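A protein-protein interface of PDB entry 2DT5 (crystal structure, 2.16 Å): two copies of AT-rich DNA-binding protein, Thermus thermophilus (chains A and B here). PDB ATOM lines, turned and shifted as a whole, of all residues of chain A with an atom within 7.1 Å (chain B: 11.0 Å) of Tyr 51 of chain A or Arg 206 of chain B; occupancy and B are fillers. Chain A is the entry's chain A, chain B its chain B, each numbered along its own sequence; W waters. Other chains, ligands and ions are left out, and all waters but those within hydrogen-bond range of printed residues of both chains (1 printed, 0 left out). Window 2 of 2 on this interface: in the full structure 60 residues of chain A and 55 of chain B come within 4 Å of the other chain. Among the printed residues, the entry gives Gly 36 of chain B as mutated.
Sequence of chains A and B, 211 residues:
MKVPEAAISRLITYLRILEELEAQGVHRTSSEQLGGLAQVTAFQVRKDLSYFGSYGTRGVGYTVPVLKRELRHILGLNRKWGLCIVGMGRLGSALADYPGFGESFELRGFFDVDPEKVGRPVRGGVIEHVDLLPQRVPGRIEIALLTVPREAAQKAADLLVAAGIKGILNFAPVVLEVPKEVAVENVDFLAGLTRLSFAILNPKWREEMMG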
ATOM      1  N   LYS A   2       0.776 -37.762  12.702  1.00  0.00           N
ATOM      2  CA  LYS A   2       2.119 -37.764  13.357  1.00  0.00           C
ATOM      3  C   LYS A   2       2.081 -36.938  14.645  1.00  0.00           C
ATOM      4  O   LYS A   2       2.124 -35.704  14.602  1.00  0.00           O
ATOM      5  CB  LYS A   2       3.161 -37.199  12.394  1.00  0.00           C
ATOM      6  N   VAL A   3       2.004 -37.622  15.786  1.00  0.00           N
ATOM      7  CA  VAL A   3       1.938 -36.946  17.087  1.00  0.00           C
ATOM      8  C   VAL A   3       3.307 -36.779  17.749  1.00  0.00           C
ATOM      9  O   VAL A   3       3.913 -37.746  18.200  1.00  0.00           O
ATOM     10  CB  VAL A   3       0.992 -37.703  18.071  1.00  0.00           C
ATOM     11  CG1 VAL A   3       0.935 -36.989  19.425  1.00  0.00           C
ATOM     12  CG2 VAL A   3      -0.403 -37.799  17.471  1.00  0.00           C
ATOM     13  N   PRO A   4       3.810 -35.539  17.814  1.00  0.00           N
ATOM     14  CA  PRO A   4       5.118 -35.278  18.433  1.00  0.00           C
ATOM     15  C   PRO A   4       5.044 -35.548  19.949  1.00  0.00           C
ATOM     16  O   PRO A   4       4.881 -34.622  20.745  1.00  0.00           O
ATOM     17  CB  PRO A   4       5.359 -33.803  18.101  1.00  0.00           C
ATOM     18  CG  PRO A   4       3.968 -33.218  18.143  1.00  0.00           C
ATOM     19  CD  PRO A   4       3.153 -34.283  17.399  1.00  0.00           C
ATOM     20  N   ALA A   7       7.579 -33.713  22.222  1.00  0.00           N
ATOM     21  CA  ALA A   7       7.328 -32.281  22.165  1.00  0.00           C
ATOM     22  C   ALA A   7       6.127 -31.933  23.042  1.00  0.00           C
ATOM     23  O   ALA A   7       6.157 -30.975  23.808  1.00  0.00           O
ATOM     24  CB  ALA A   7       7.077 -31.846  20.719  1.00  0.00           C
ATOM     25  N   ILE A   8       5.081 -32.737  22.934  1.00  0.00           N
ATOM     26  CA  ILE A   8       3.872 -32.537  23.713  1.00  0.00           C
ATOM     27  C   ILE A   8       4.193 -32.640  25.193  1.00  0.00           C
ATOM     28  O   ILE A   8       3.773 -31.786  25.977  1.00  0.00           O
ATOM     29  CB  ILE A   8       2.817 -33.598  23.376  1.00  0.00           C
ATOM     30  CG1 ILE A   8       2.375 -33.448  21.921  1.00  0.00           C
ATOM     31  CG2 ILE A   8       1.614 -33.470  24.317  1.00  0.00           C
ATOM     32  CD1 ILE A   8       1.552 -32.235  21.659  1.00  0.00           C
ATOM     33  N   LEU A  11       5.584 -29.526  26.151  1.00  0.00           N
ATOM     34  CA  LEU A  11       4.612 -28.422  26.213  1.00  0.00           C
ATOM     35  C   LEU A  11       3.845 -28.444  27.525  1.00  0.00           C
ATOM     36  O   LEU A  11       3.559 -27.402  28.114  1.00  0.00           O
ATOM     37  CB  LEU A  11       3.584 -28.510  25.088  1.00  0.00           C
ATOM     38  CG  LEU A  11       3.947 -27.947  23.727  1.00  0.00           C
ATOM     39  CD1 LEU A  11       2.717 -28.041  22.848  1.00  0.00           C
ATOM     40  CD2 LEU A  11       4.402 -26.496  23.851  1.00  0.00           C
ATOM     41  N   GLN A  44      16.012 -24.595  23.006  1.00  0.00           N
ATOM     42  CA  GLN A  44      15.004 -25.644  22.824  1.00  0.00           C
ATOM     43  C   GLN A  44      13.581 -25.127  23.105  1.00  0.00           C
ATOM     44  O   GLN A  44      12.633 -25.439  22.374  1.00  0.00           O
ATOM     45  CB  GLN A  44      15.298 -26.835  23.736  1.00  0.00           C
ATOM     46  CG  GLN A  44      14.290 -27.978  23.578  1.00  0.00           C
ATOM     47  CD  GLN A  44      14.149 -28.412  22.124  1.00  0.00           C
ATOM     48  OE1 GLN A  44      15.125 -28.804  21.487  1.00  0.00           O
ATOM     49  NE2 GLN A  44      12.936 -28.330  21.593  1.00  0.00           N
ATOM     50  N   VAL A  45      13.433 -24.346  24.174  1.00  0.00           N
ATOM     51  CA  VAL A  45      12.124 -23.791  24.511  1.00  0.00           C
ATOM     52  C   VAL A  45      11.612 -22.948  23.348  1.00  0.00           C
ATOM     53  O   VAL A  45      10.485 -23.127  22.903  1.00  0.00           O
ATOM     54  CB  VAL A  45      12.203 -22.914  25.767  1.00  0.00           C
ATOM     55  CG1 VAL A  45      10.878 -22.161  25.971  1.00  0.00           C
ATOM     56  CG2 VAL A  45      12.521 -23.796  26.983  1.00  0.00           C
ATOM     57  N   ARG A  46      12.444 -22.020  22.862  1.00  0.00           N
ATOM     58  CA  ARG A  46      12.063 -21.161  21.735  1.00  0.00           C
ATOM     59  C   ARG A  46      11.663 -22.021  20.547  1.00  0.00           C
ATOM     60  O   ARG A  46      10.696 -21.726  19.842  1.00  0.00           O
ATOM     61  CB  ARG A  46      13.227 -20.242  21.311  1.00  0.00           C
ATOM     62  CG  ARG A  46      13.613 -19.159  22.325  1.00  0.00           C
ATOM     63  CD  ARG A  46      14.556 -18.122  21.707  1.00  0.00           C
ATOM     64  NE  ARG A  46      15.894 -18.650  21.432  1.00  0.00           N
ATOM     65  CZ  ARG A  46      16.904 -18.660  22.308  1.00  0.00           C
ATOM     66  NH1 ARG A  46      16.736 -18.170  23.537  1.00  0.00           N
ATOM     67  NH2 ARG A  46      18.096 -19.144  21.952  1.00  0.00           N
ATOM     68  N   LYS A  47      12.410 -23.098  20.339  1.00  0.00           N
ATOM     69  CA  LYS A  47      12.156 -23.988  19.221  1.00  0.00           C
ATOM     70  C   LYS A  47      10.817 -24.722  19.349  1.00  0.00           C
ATOM     71  O   LYS A  47      10.040 -24.786  18.393  1.00  0.00           O
ATOM     72  CB  LYS A  47      13.313 -24.981  19.081  1.00  0.00           C
ATOM     73  CG  LYS A  47      13.208 -25.843  17.823  1.00  0.00           C
ATOM     74  CD  LYS A  47      14.519 -26.541  17.468  1.00  0.00           C
ATOM     75  CE  LYS A  47      14.383 -27.263  16.126  1.00  0.00           C
ATOM     76  NZ  LYS A  47      15.669 -27.838  15.620  1.00  0.00           N
ATOM     77  N   ASP A  48      10.546 -25.269  20.530  1.00  0.00           N
ATOM     78  CA  ASP A  48       9.284 -25.970  20.753  1.00  0.00           C
ATOM     79  C   ASP A  48       8.108 -25.029  20.570  1.00  0.00           C
ATOM     80  O   ASP A  48       7.149 -25.345  19.864  1.00  0.00           O
ATOM     81  CB  ASP A  48       9.218 -26.546  22.168  1.00  0.00           C
ATOM     82  CG  ASP A  48      10.135 -27.735  22.359  1.00  0.00           C
ATOM     83  OD1 ASP A  48      10.338 -28.496  21.385  1.00  0.00           O
ATOM     84  OD2 ASP A  48      10.633 -27.913  23.492  1.00  0.00           O
ATOM     85  N   LEU A  49       8.182 -23.865  21.212  1.00  0.00           N
ATOM     86  CA  LEU A  49       7.085 -22.906  21.112  1.00  0.00           C
ATOM     87  C   LEU A  49       6.781 -22.503  19.665  1.00  0.00           C
ATOM     88  O   LEU A  49       5.614 -22.445  19.257  1.00  0.00           O
ATOM     89  CB  LEU A  49       7.389 -21.690  21.990  1.00  0.00           C
ATOM     90  CG  LEU A  49       7.313 -22.058  23.481  1.00  0.00           C
ATOM     91  CD1 LEU A  49       7.503 -20.800  24.337  1.00  0.00           C
ATOM     92  CD2 LEU A  49       5.935 -22.722  23.771  1.00  0.00           C
ATOM     93  N   SER A  50       7.838 -22.232  18.894  1.00  0.00           N
ATOM     94  CA  SER A  50       7.705 -21.858  17.478  1.00  0.00           C
ATOM     95  C   SER A  50       7.134 -23.068  16.734  1.00  0.00           C
ATOM     96  O   SER A  50       6.235 -22.923  15.905  1.00  0.00           O
ATOM     97  CB  SER A  50       9.090 -21.486  16.892  1.00  0.00           C
ATOM     98  OG  SER A  50       9.596 -20.272  17.454  1.00  0.00           O
ATOM     99  N   TYR A  51       7.664 -24.256  17.048  1.00  0.00           N
ATOM    100  CA  TYR A  51       7.204 -25.505  16.428  1.00  0.00           C
ATOM    101  C   TYR A  51       5.688 -25.610  16.532  1.00  0.00           C
ATOM    102  O   TYR A  51       5.030 -26.142  15.627  1.00  0.00           O
ATOM    103  CB  TYR A  51       7.854 -26.728  17.109  1.00  0.00           C
ATOM    104  CG  TYR A  51       7.315 -28.074  16.628  1.00  0.00           C
ATOM    105  CD1 TYR A  51       7.725 -28.630  15.412  1.00  0.00           C
ATOM    106  CD2 TYR A  51       6.348 -28.765  17.371  1.00  0.00           C
ATOM    107  CE1 TYR A  51       7.179 -29.839  14.945  1.00  0.00           C
ATOM    108  CE2 TYR A  51       5.798 -29.966  16.916  1.00  0.00           C
ATOM    109  CZ  TYR A  51       6.211 -30.499  15.704  1.00  0.00           C
ATOM    110  OH  TYR A  51       5.628 -31.665  15.247  1.00  0.00           O
ATOM    111  N   PHE A  52       5.140 -25.106  17.646  1.00  0.00           N
ATOM    112  CA  PHE A  52       3.697 -25.130  17.871  1.00  0.00           C
ATOM    113  C   PHE A  52       2.964 -23.829  17.535  1.00  0.00           C
ATOM    114  O   PHE A  52       1.781 -23.695  17.851  1.00  0.00           O
ATOM    115  CB  PHE A  52       3.378 -25.527  19.317  1.00  0.00           C
ATOM    116  CG  PHE A  52       3.605 -26.978  19.606  1.00  0.00           C
ATOM    117  CD1 PHE A  52       4.752 -27.401  20.286  1.00  0.00           C
ATOM    118  CD2 PHE A  52       2.696 -27.936  19.158  1.00  0.00           C
ATOM    119  CE1 PHE A  52       4.999 -28.768  20.516  1.00  0.00           C
ATOM    120  CE2 PHE A  52       2.927 -29.302  19.382  1.00  0.00           C
ATOM    121  CZ  PHE A  52       4.083 -29.722  20.063  1.00  0.00           C
ATOM    122  N   GLY A  53       3.658 -22.874  16.921  1.00  0.00           N
ATOM    123  CA  GLY A  53       3.003 -21.621  16.554  1.00  0.00           C
ATOM    124  C   GLY A  53       3.110 -20.403  17.478  1.00  0.00           C
ATOM    125  O   GLY A  53       2.598 -19.335  17.136  1.00  0.00           O
ATOM    126  N   SER A  54       3.754 -20.539  18.639  1.00  0.00           N
ATOM    127  CA  SER A  54       3.903 -19.413  19.580  1.00  0.00           C
ATOM    128  C   SER A  54       5.287 -18.816  19.412  1.00  0.00           C
ATOM    129  O   SER A  54       6.284 -19.363  19.906  1.00  0.00           O
ATOM    130  CB  SER A  54       3.729 -19.881  21.032  1.00  0.00           C
ATOM    131  OG  SER A  54       2.383 -20.247  21.284  1.00  0.00           O
ATOM    132  N   TYR A  55       5.346 -17.683  18.724  1.00  0.00           N
ATOM    133  CA  TYR A  55       6.624 -17.029  18.446  1.00  0.00           C
ATOM    134  C   TYR A  55       6.971 -16.051  19.558  1.00  0.00           C
ATOM    135  O   TYR A  55       6.085 -15.514  20.218  1.00  0.00           O
ATOM    136  CB  TYR A  55       6.552 -16.328  17.075  1.00  0.00           C
ATOM    137  CG  TYR A  55       6.153 -17.267  15.941  1.00  0.00           C
ATOM    138  CD1 TYR A  55       5.092 -16.959  15.084  1.00  0.00           C
ATOM    139  CD2 TYR A  55       6.819 -18.475  15.747  1.00  0.00           C
ATOM    140  CE1 TYR A  55       4.712 -17.833  14.066  1.00  0.00           C
ATOM    141  CE2 TYR A  55       6.443 -19.359  14.737  1.00  0.00           C
ATOM    142  CZ  TYR A  55       5.392 -19.035  13.900  1.00  0.00           C
ATOM    143  OH  TYR A  55       5.024 -19.927  12.907  1.00  0.00           O
ATOM    144  N   GLY B  35      15.721 -40.644  12.365  1.00  0.00           N
ATOM    145  CA  GLY B  35      15.311 -39.356  12.885  1.00  0.00           C
ATOM    146  C   GLY B  35      13.885 -39.016  12.518  1.00  0.00           C
ATOM    147  O   GLY B  35      13.152 -38.430  13.315  1.00  0.00           O
ATOM    148  N   GLY B  36      13.500 -39.384  11.301  1.00  0.00           N
ATOM    149  CA  GLY B  36      12.159 -39.111  10.821  1.00  0.00           C
ATOM    150  C   GLY B  36      11.140 -39.952  11.555  1.00  0.00           C
ATOM    151  O   GLY B  36      10.156 -39.431  12.069  1.00  0.00           O
ATOM    152  N   ALA B  38      11.342 -41.265  14.400  1.00  0.00           N
ATOM    153  CA  ALA B  38      11.295 -40.951  15.827  1.00  0.00           C
ATOM    154  C   ALA B  38      10.996 -39.477  16.053  1.00  0.00           C
ATOM    155  O   ALA B  38      10.963 -39.011  17.188  1.00  0.00           O
ATOM    156  CB  ALA B  38      12.628 -41.317  16.485  1.00  0.00           C
ATOM    157  N   GLN B  39      10.802 -38.745  14.964  1.00  0.00           N
ATOM    158  CA  GLN B  39      10.518 -37.320  15.025  1.00  0.00           C
ATOM    159  C   GLN B  39      11.628 -36.517  15.703  1.00  0.00           C
ATOM    160  O   GLN B  39      11.369 -35.628  16.517  1.00  0.00           O
ATOM    161  CB  GLN B  39       9.182 -37.067  15.734  1.00  0.00           C
ATOM    162  CG  GLN B  39       8.028 -37.894  15.172  1.00  0.00           C
ATOM    163  CD  GLN B  39       6.655 -37.375  15.593  1.00  0.00           C
ATOM    164  OE1 GLN B  39       5.688 -38.138  15.666  1.00  0.00           O
ATOM    165  NE2 GLN B  39       6.562 -36.072  15.858  1.00  0.00           N
ATOM    166  N   VAL B  40      12.869 -36.834  15.358  1.00  0.00           N
ATOM    167  CA  VAL B  40      14.014 -36.114  15.898  1.00  0.00           C
ATOM    168  C   VAL B  40      14.966 -35.887  14.721  1.00  0.00           C
ATOM    169  O   VAL B  40      15.027 -36.710  13.813  1.00  0.00           O
ATOM    170  CB  VAL B  40      14.734 -36.931  17.020  1.00  0.00           C
ATOM    171  CG1 VAL B  40      13.710 -37.529  17.989  1.00  0.00           C
ATOM    172  CG2 VAL B  40      15.571 -38.021  16.417  1.00  0.00           C
ATOM    173  N   THR B  41      15.705 -34.780  14.737  1.00  0.00           N
ATOM    174  CA  THR B  41      16.626 -34.465  13.655  1.00  0.00           C
ATOM    175  C   THR B  41      17.690 -35.552  13.479  1.00  0.00           C
ATOM    176  O   THR B  41      18.118 -36.188  14.444  1.00  0.00           O
ATOM    177  CB  THR B  41      17.338 -33.102  13.891  1.00  0.00           C
ATOM    178  OG1 THR B  41      18.272 -33.220  14.970  1.00  0.00           O
ATOM    179  CG2 THR B  41      16.323 -32.014  14.252  1.00  0.00           C
ATOM    180  N   PHE B 198      -5.038 -33.394  21.672  1.00  0.00           N
ATOM    181  CA  PHE B 198      -4.242 -32.668  20.689  1.00  0.00           C
ATOM    182  C   PHE B 198      -4.511 -33.230  19.295  1.00  0.00           C
ATOM    183  O   PHE B 198      -4.772 -32.484  18.352  1.00  0.00           O
ATOM    184  CB  PHE B 198      -2.742 -32.783  20.990  1.00  0.00           C
ATOM    185  CG  PHE B 198      -1.868 -32.243  19.894  1.00  0.00           C
ATOM    186  CD1 PHE B 198      -1.635 -30.880  19.780  1.00  0.00           C
ATOM    187  CD2 PHE B 198      -1.349 -33.091  18.920  1.00  0.00           C
ATOM    188  CE1 PHE B 198      -0.906 -30.368  18.712  1.00  0.00           C
ATOM    189  CE2 PHE B 198      -0.619 -32.584  17.845  1.00  0.00           C
ATOM    190  CZ  PHE B 198      -0.399 -31.221  17.740  1.00  0.00           C
ATOM    191  N   ALA B 199      -4.446 -34.554  19.172  1.00  0.00           N
ATOM    192  CA  ALA B 199      -4.670 -35.217  17.897  1.00  0.00           C
ATOM    193  C   ALA B 199      -6.068 -34.959  17.328  1.00  0.00           C
ATOM    194  O   ALA B 199      -6.218 -34.673  16.143  1.00  0.00           O
ATOM    195  CB  ALA B 199      -4.428 -36.716  18.050  1.00  0.00           C
ATOM    196  N   LEU B 201      -8.045 -32.427  17.877  1.00  0.00           N
ATOM    197  CA  LEU B 201      -8.187 -31.031  17.464  1.00  0.00           C
ATOM    198  C   LEU B 201      -7.226 -30.634  16.340  1.00  0.00           C
ATOM    199  O   LEU B 201      -7.453 -29.635  15.661  1.00  0.00           O
ATOM    200  CB  LEU B 201      -7.978 -30.097  18.654  1.00  0.00           C
ATOM    201  CG  LEU B 201      -8.904 -30.341  19.841  1.00  0.00           C
ATOM    202  CD1 LEU B 201      -8.560 -29.354  20.926  1.00  0.00           C
ATOM    203  CD2 LEU B 201     -10.363 -30.199  19.417  1.00  0.00           C
ATOM    204  N   ASN B 202      -6.154 -31.395  16.147  1.00  0.00           N
ATOM    205  CA  ASN B 202      -5.201 -31.080  15.073  1.00  0.00           C
ATOM    206  C   ASN B 202      -4.995 -32.342  14.239  1.00  0.00           C
ATOM    207  O   ASN B 202      -3.886 -32.873  14.132  1.00  0.00           O
ATOM    208  CB  ASN B 202      -3.872 -30.597  15.668  1.00  0.00           C
ATOM    209  CG  ASN B 202      -4.047 -29.380  16.568  1.00  0.00           C
ATOM    210  OD1 ASN B 202      -4.366 -29.500  17.765  1.00  0.00           O
ATOM    211  ND2 ASN B 202      -3.858 -28.199  15.993  1.00  0.00           N
ATOM    212  N   PRO B 203      -6.074 -32.828  13.614  1.00  0.00           N
ATOM    213  CA  PRO B 203      -6.068 -34.039  12.785  1.00  0.00           C
ATOM    214  C   PRO B 203      -5.033 -34.143  11.668  1.00  0.00           C
ATOM    215  O   PRO B 203      -4.588 -35.242  11.340  1.00  0.00           O
ATOM    216  CB  PRO B 203      -7.491 -34.083  12.237  1.00  0.00           C
ATOM    217  CG  PRO B 203      -7.819 -32.629  12.070  1.00  0.00           C
ATOM    218  CD  PRO B 203      -7.316 -32.060  13.393  1.00  0.00           C
ATOM    219  N   LYS B 204      -4.655 -33.012  11.087  1.00  0.00           N
ATOM    220  CA  LYS B 204      -3.708 -33.010   9.977  1.00  0.00           C
ATOM    221  C   LYS B 204      -2.375 -32.369  10.361  1.00  0.00           C
ATOM    222  O   LYS B 204      -1.615 -31.933   9.494  1.00  0.00           O
ATOM    223  CB  LYS B 204      -4.317 -32.236   8.807  1.00  0.00           C
ATOM    224  CG  LYS B 204      -5.779 -32.573   8.515  1.00  0.00           C
ATOM    225  CD  LYS B 204      -5.919 -33.879   7.748  1.00  0.00           C
ATOM    226  CE  LYS B 204      -5.358 -33.754   6.335  1.00  0.00           C
ATOM    227  NZ  LYS B 204      -5.646 -34.948   5.490  1.00  0.00           N
ATOM    228  N   TRP B 205      -2.100 -32.319  11.658  1.00  0.00           N
ATOM    229  CA  TRP B 205      -0.877 -31.711  12.182  1.00  0.00           C
ATOM    230  C   TRP B 205       0.393 -31.865  11.347  1.00  0.00           C
ATOM    231  O   TRP B 205       0.884 -32.976  11.167  1.00  0.00           O
ATOM    232  CB  TRP B 205      -0.583 -32.244  13.581  1.00  0.00           C
ATOM    233  CG  TRP B 205       0.599 -31.581  14.198  1.00  0.00           C
ATOM    234  CD1 TRP B 205       1.746 -32.180  14.651  1.00  0.00           C
ATOM    235  CD2 TRP B 205       0.759 -30.179  14.427  1.00  0.00           C
ATOM    236  NE1 TRP B 205       2.607 -31.232  15.154  1.00  0.00           N
ATOM    237  CE2 TRP B 205       2.024 -29.997  15.036  1.00  0.00           C
ATOM    238  CE3 TRP B 205      -0.054 -29.058  14.195  1.00  0.00           C
ATOM    239  CZ2 TRP B 205       2.508 -28.733  15.393  1.00  0.00           C
ATOM    240  CZ3 TRP B 205       0.426 -27.800  14.552  1.00  0.00           C
ATOM    241  CH2 TRP B 205       1.693 -27.649  15.152  1.00  0.00           C
ATOM    242  N   ARG B 206       0.911 -30.741  10.844  1.00  0.00           N
ATOM    243  CA  ARG B 206       2.157 -30.718  10.077  1.00  0.00           C
ATOM    244  C   ARG B 206       2.221 -31.536   8.785  1.00  0.00           C
ATOM    245  O   ARG B 206       3.305 -31.706   8.226  1.00  0.00           O
ATOM    246  CB  ARG B 206       3.321 -31.170  10.969  1.00  0.00           C
ATOM    247  CG  ARG B 206       4.268 -30.078  11.475  1.00  0.00           C
ATOM    248  CD  ARG B 206       3.555 -29.094  12.362  1.00  0.00           C
ATOM    249  NE  ARG B 206       4.445 -28.211  13.125  1.00  0.00           N
ATOM    250  CZ  ARG B 206       5.536 -27.601  12.654  1.00  0.00           C
ATOM    251  NH1 ARG B 206       5.940 -27.768  11.395  1.00  0.00           N
ATOM    252  NH2 ARG B 206       6.202 -26.767  13.440  1.00  0.00           N
ATOM    253  N   GLU B 207       1.101 -32.056   8.300  1.00  0.00           N
ATOM    254  CA  GLU B 207       1.164 -32.836   7.069  1.00  0.00           C
ATOM    255  C   GLU B 207       1.556 -31.961   5.879  1.00  0.00           C
ATOM    256  O   GLU B 207       1.549 -30.730   5.972  1.00  0.00           O
ATOM    257  CB  GLU B 207      -0.172 -33.541   6.813  1.00  0.00           C
ATOM    258  CG  GLU B 207      -0.448 -34.649   7.835  1.00  0.00           C
ATOM    259  CD  GLU B 207      -1.744 -35.414   7.590  1.00  0.00           C
ATOM    260  OE1 GLU B 207      -2.042 -36.326   8.388  1.00  0.00           O
ATOM    261  OE2 GLU B 207      -2.461 -35.109   6.611  1.00  0.00           O
ATOM    262  N   GLU B 208       1.935 -32.602   4.775  1.00  0.00           N
ATOM    263  CA  GLU B 208       2.321 -31.885   3.560  1.00  0.00           C
ATOM    264  C   GLU B 208       1.126 -31.050   3.110  1.00  0.00           C
ATOM    265  O   GLU B 208       1.281 -29.937   2.603  1.00  0.00           O
ATOM    266  CB  GLU B 208       2.719 -32.876   2.460  1.00  0.00           C
ATOM    267  CG  GLU B 208       3.941 -33.729   2.796  1.00  0.00           C
ATOM    268  CD  GLU B 208       5.257 -32.978   2.644  1.00  0.00           C
ATOM    269  OE1 GLU B 208       5.371 -31.842   3.163  1.00  0.00           O
ATOM    270  OE2 GLU B 208       6.182 -33.535   2.009  1.00  0.00           O
ATOM    271  N   MET B 209      -0.065 -31.610   3.302  1.00  0.00           N
ATOM    272  CA  MET B 209      -1.312 -30.940   2.961  1.00  0.00           C
ATOM    273  C   MET B 209      -2.342 -31.224   4.060  1.00  0.00           C
ATOM    274  O   MET B 209      -2.728 -32.374   4.288  1.00  0.00           O
ATOM    275  CB  MET B 209      -1.833 -31.426   1.600  1.00  0.00           C
ATOM    276  CG  MET B 209      -3.171 -30.812   1.185  1.00  0.00           C
ATOM    277  SD  MET B 209      -3.179 -28.994   1.119  1.00  0.00           S
ATOM    278  CE  MET B 209      -3.008 -28.718  -0.641  1.00  0.00           C
ATOM    279  N   MET B 210      -2.763 -30.167   4.753  1.00  0.00           N
ATOM    280  CA  MET B 210      -3.739 -30.282   5.829  1.00  0.00           C
ATOM    281  C   MET B 210      -5.137 -29.945   5.314  1.00  0.00           C
ATOM    282  O   MET B 210      -6.137 -30.312   5.927  1.00  0.00           O
ATOM    283  CB  MET B 210      -3.372 -29.345   6.990  1.00  0.00           C
ATOM    284  CG  MET B 210      -1.942 -29.499   7.498  1.00  0.00           C
ATOM    285  SD  MET B 210      -1.594 -28.586   9.028  1.00  0.00           S
ATOM    286  CE  MET B 210      -2.174 -26.951   8.604  1.00  0.00           C
ATOM    287  N   GLY B 211      -5.197 -29.243   4.186  1.00  0.00           N
ATOM    288  CA  GLY B 211      -6.479 -28.880   3.610  1.00  0.00           C
ATOM    289  C   GLY B 211      -7.123 -30.047   2.883  1.00  0.00           C
ATOM    290  O   GLY B 211      -7.359 -29.938   1.661  1.00  0.00           O
ATOM    291  OXT GLY B 211      -7.396 -31.079   3.534  1.00  0.00           O
HETATM  292  O   HOH W   1      -0.294 -35.920  11.395  1.00  0.00           O
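The backbone carbonyl oxygen (O) of Phe 198 of chain B sits close to the side-chain amide oxygen (OD1) of Asn 202 of chain B (3.1 Å). The side-chain sulfur (SD) of Met 210 of chain B is in hydrogen-bond range of the backbone NH (N) of Arg 206 of chain B (3.8 Å).
No position is printed for both chains. Of the 9 pairs that touch across the chains among the printed residues, none has its exchanged pair printed and touching as well.
Hydrophobic or aromatic side chains of chain A within 4 Å of the printed part of chain B: Pro 4, Ile 8, Tyr 51 and Phe 52. Along chain A the printed residues that touch a printed residue of chain B span positions 2 to 52. Among the printed residues, 9 pairs touch across the chains. Among the printed residues, no Asp or Glu carboxylate lies within 4 Å of a Lys or Arg side-chain nitrogen of the other chain.
Among the printed residues, pairs that only touch across the chains: Lys 2 of chain A with Trp 205 of chain B (3.5 Å), Pro 4 of chain A with Trp 205 of chain B (3.7 Å), Ile 8 of chain A with Phe 198 of chain B (3.8 Å), Phe 52 of chain A with Trp 205 of chain B (3.9 Å) and Lys 2 of chain A with Gln 39 of chain B (3.9 Å).
The side-chain amide oxygen of Gln 39 of chain B sits close to the backbone carbonyl oxygen of Val 3 of chain A, 3.1 Å away. The side-chain hydroxyl of Tyr 51 of chain A sits at hydrogen-bond distance from the indole nitrogen of Trp 205 of chain B (3.1 Å). The backbone carbonyl oxygen of Tyr 51 of chain A sits at hydrogen-bond distance from the guanidinium group of Arg 206 of chain B, 2.6 Å away. N of Pro 4 of chain A lies close to NE2 of Gln 39 of chain B, at 3.4 Å.
Water W1 lies within hydrogen-bond range of N of Lys 2 of chain A (2.5 Å) and O of Trp 205 of chain B (3.2 Å).
Printed residues of chain A within 4 Å of Arg 206 of chain B: Tyr 51. Of chain B, only Gln 39 and Trp 205 come within 4 Å of Pro 4 of chain A. Phe 52 of chain A touches just one residue of chain B: Trp 205 (3.9 Å). Of the printed residues of chain A, Trp 205 of chain B touches Lys 2 (3.5 Å), Pro 4 (3.7 Å), Tyr 51 (3.1 Å) and Phe 52 (3.9 Å). Of the printed residues of chain B, Val 3 of chain A touches Gln 39 (3.1 Å). Of the printed residues of chain A, Phe 198 of chain B touches Ile 8. Asp 48 of chain A touches none of the printed residues of chain B. The nearest residue of chain B that does not touch Tyr 51 of chain A is Gln 39 of chain B (4.5 Å). The nearest residue of chain A that does not touch Arg 206 of chain B is Ser 50 of chain A (4.6 Å).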
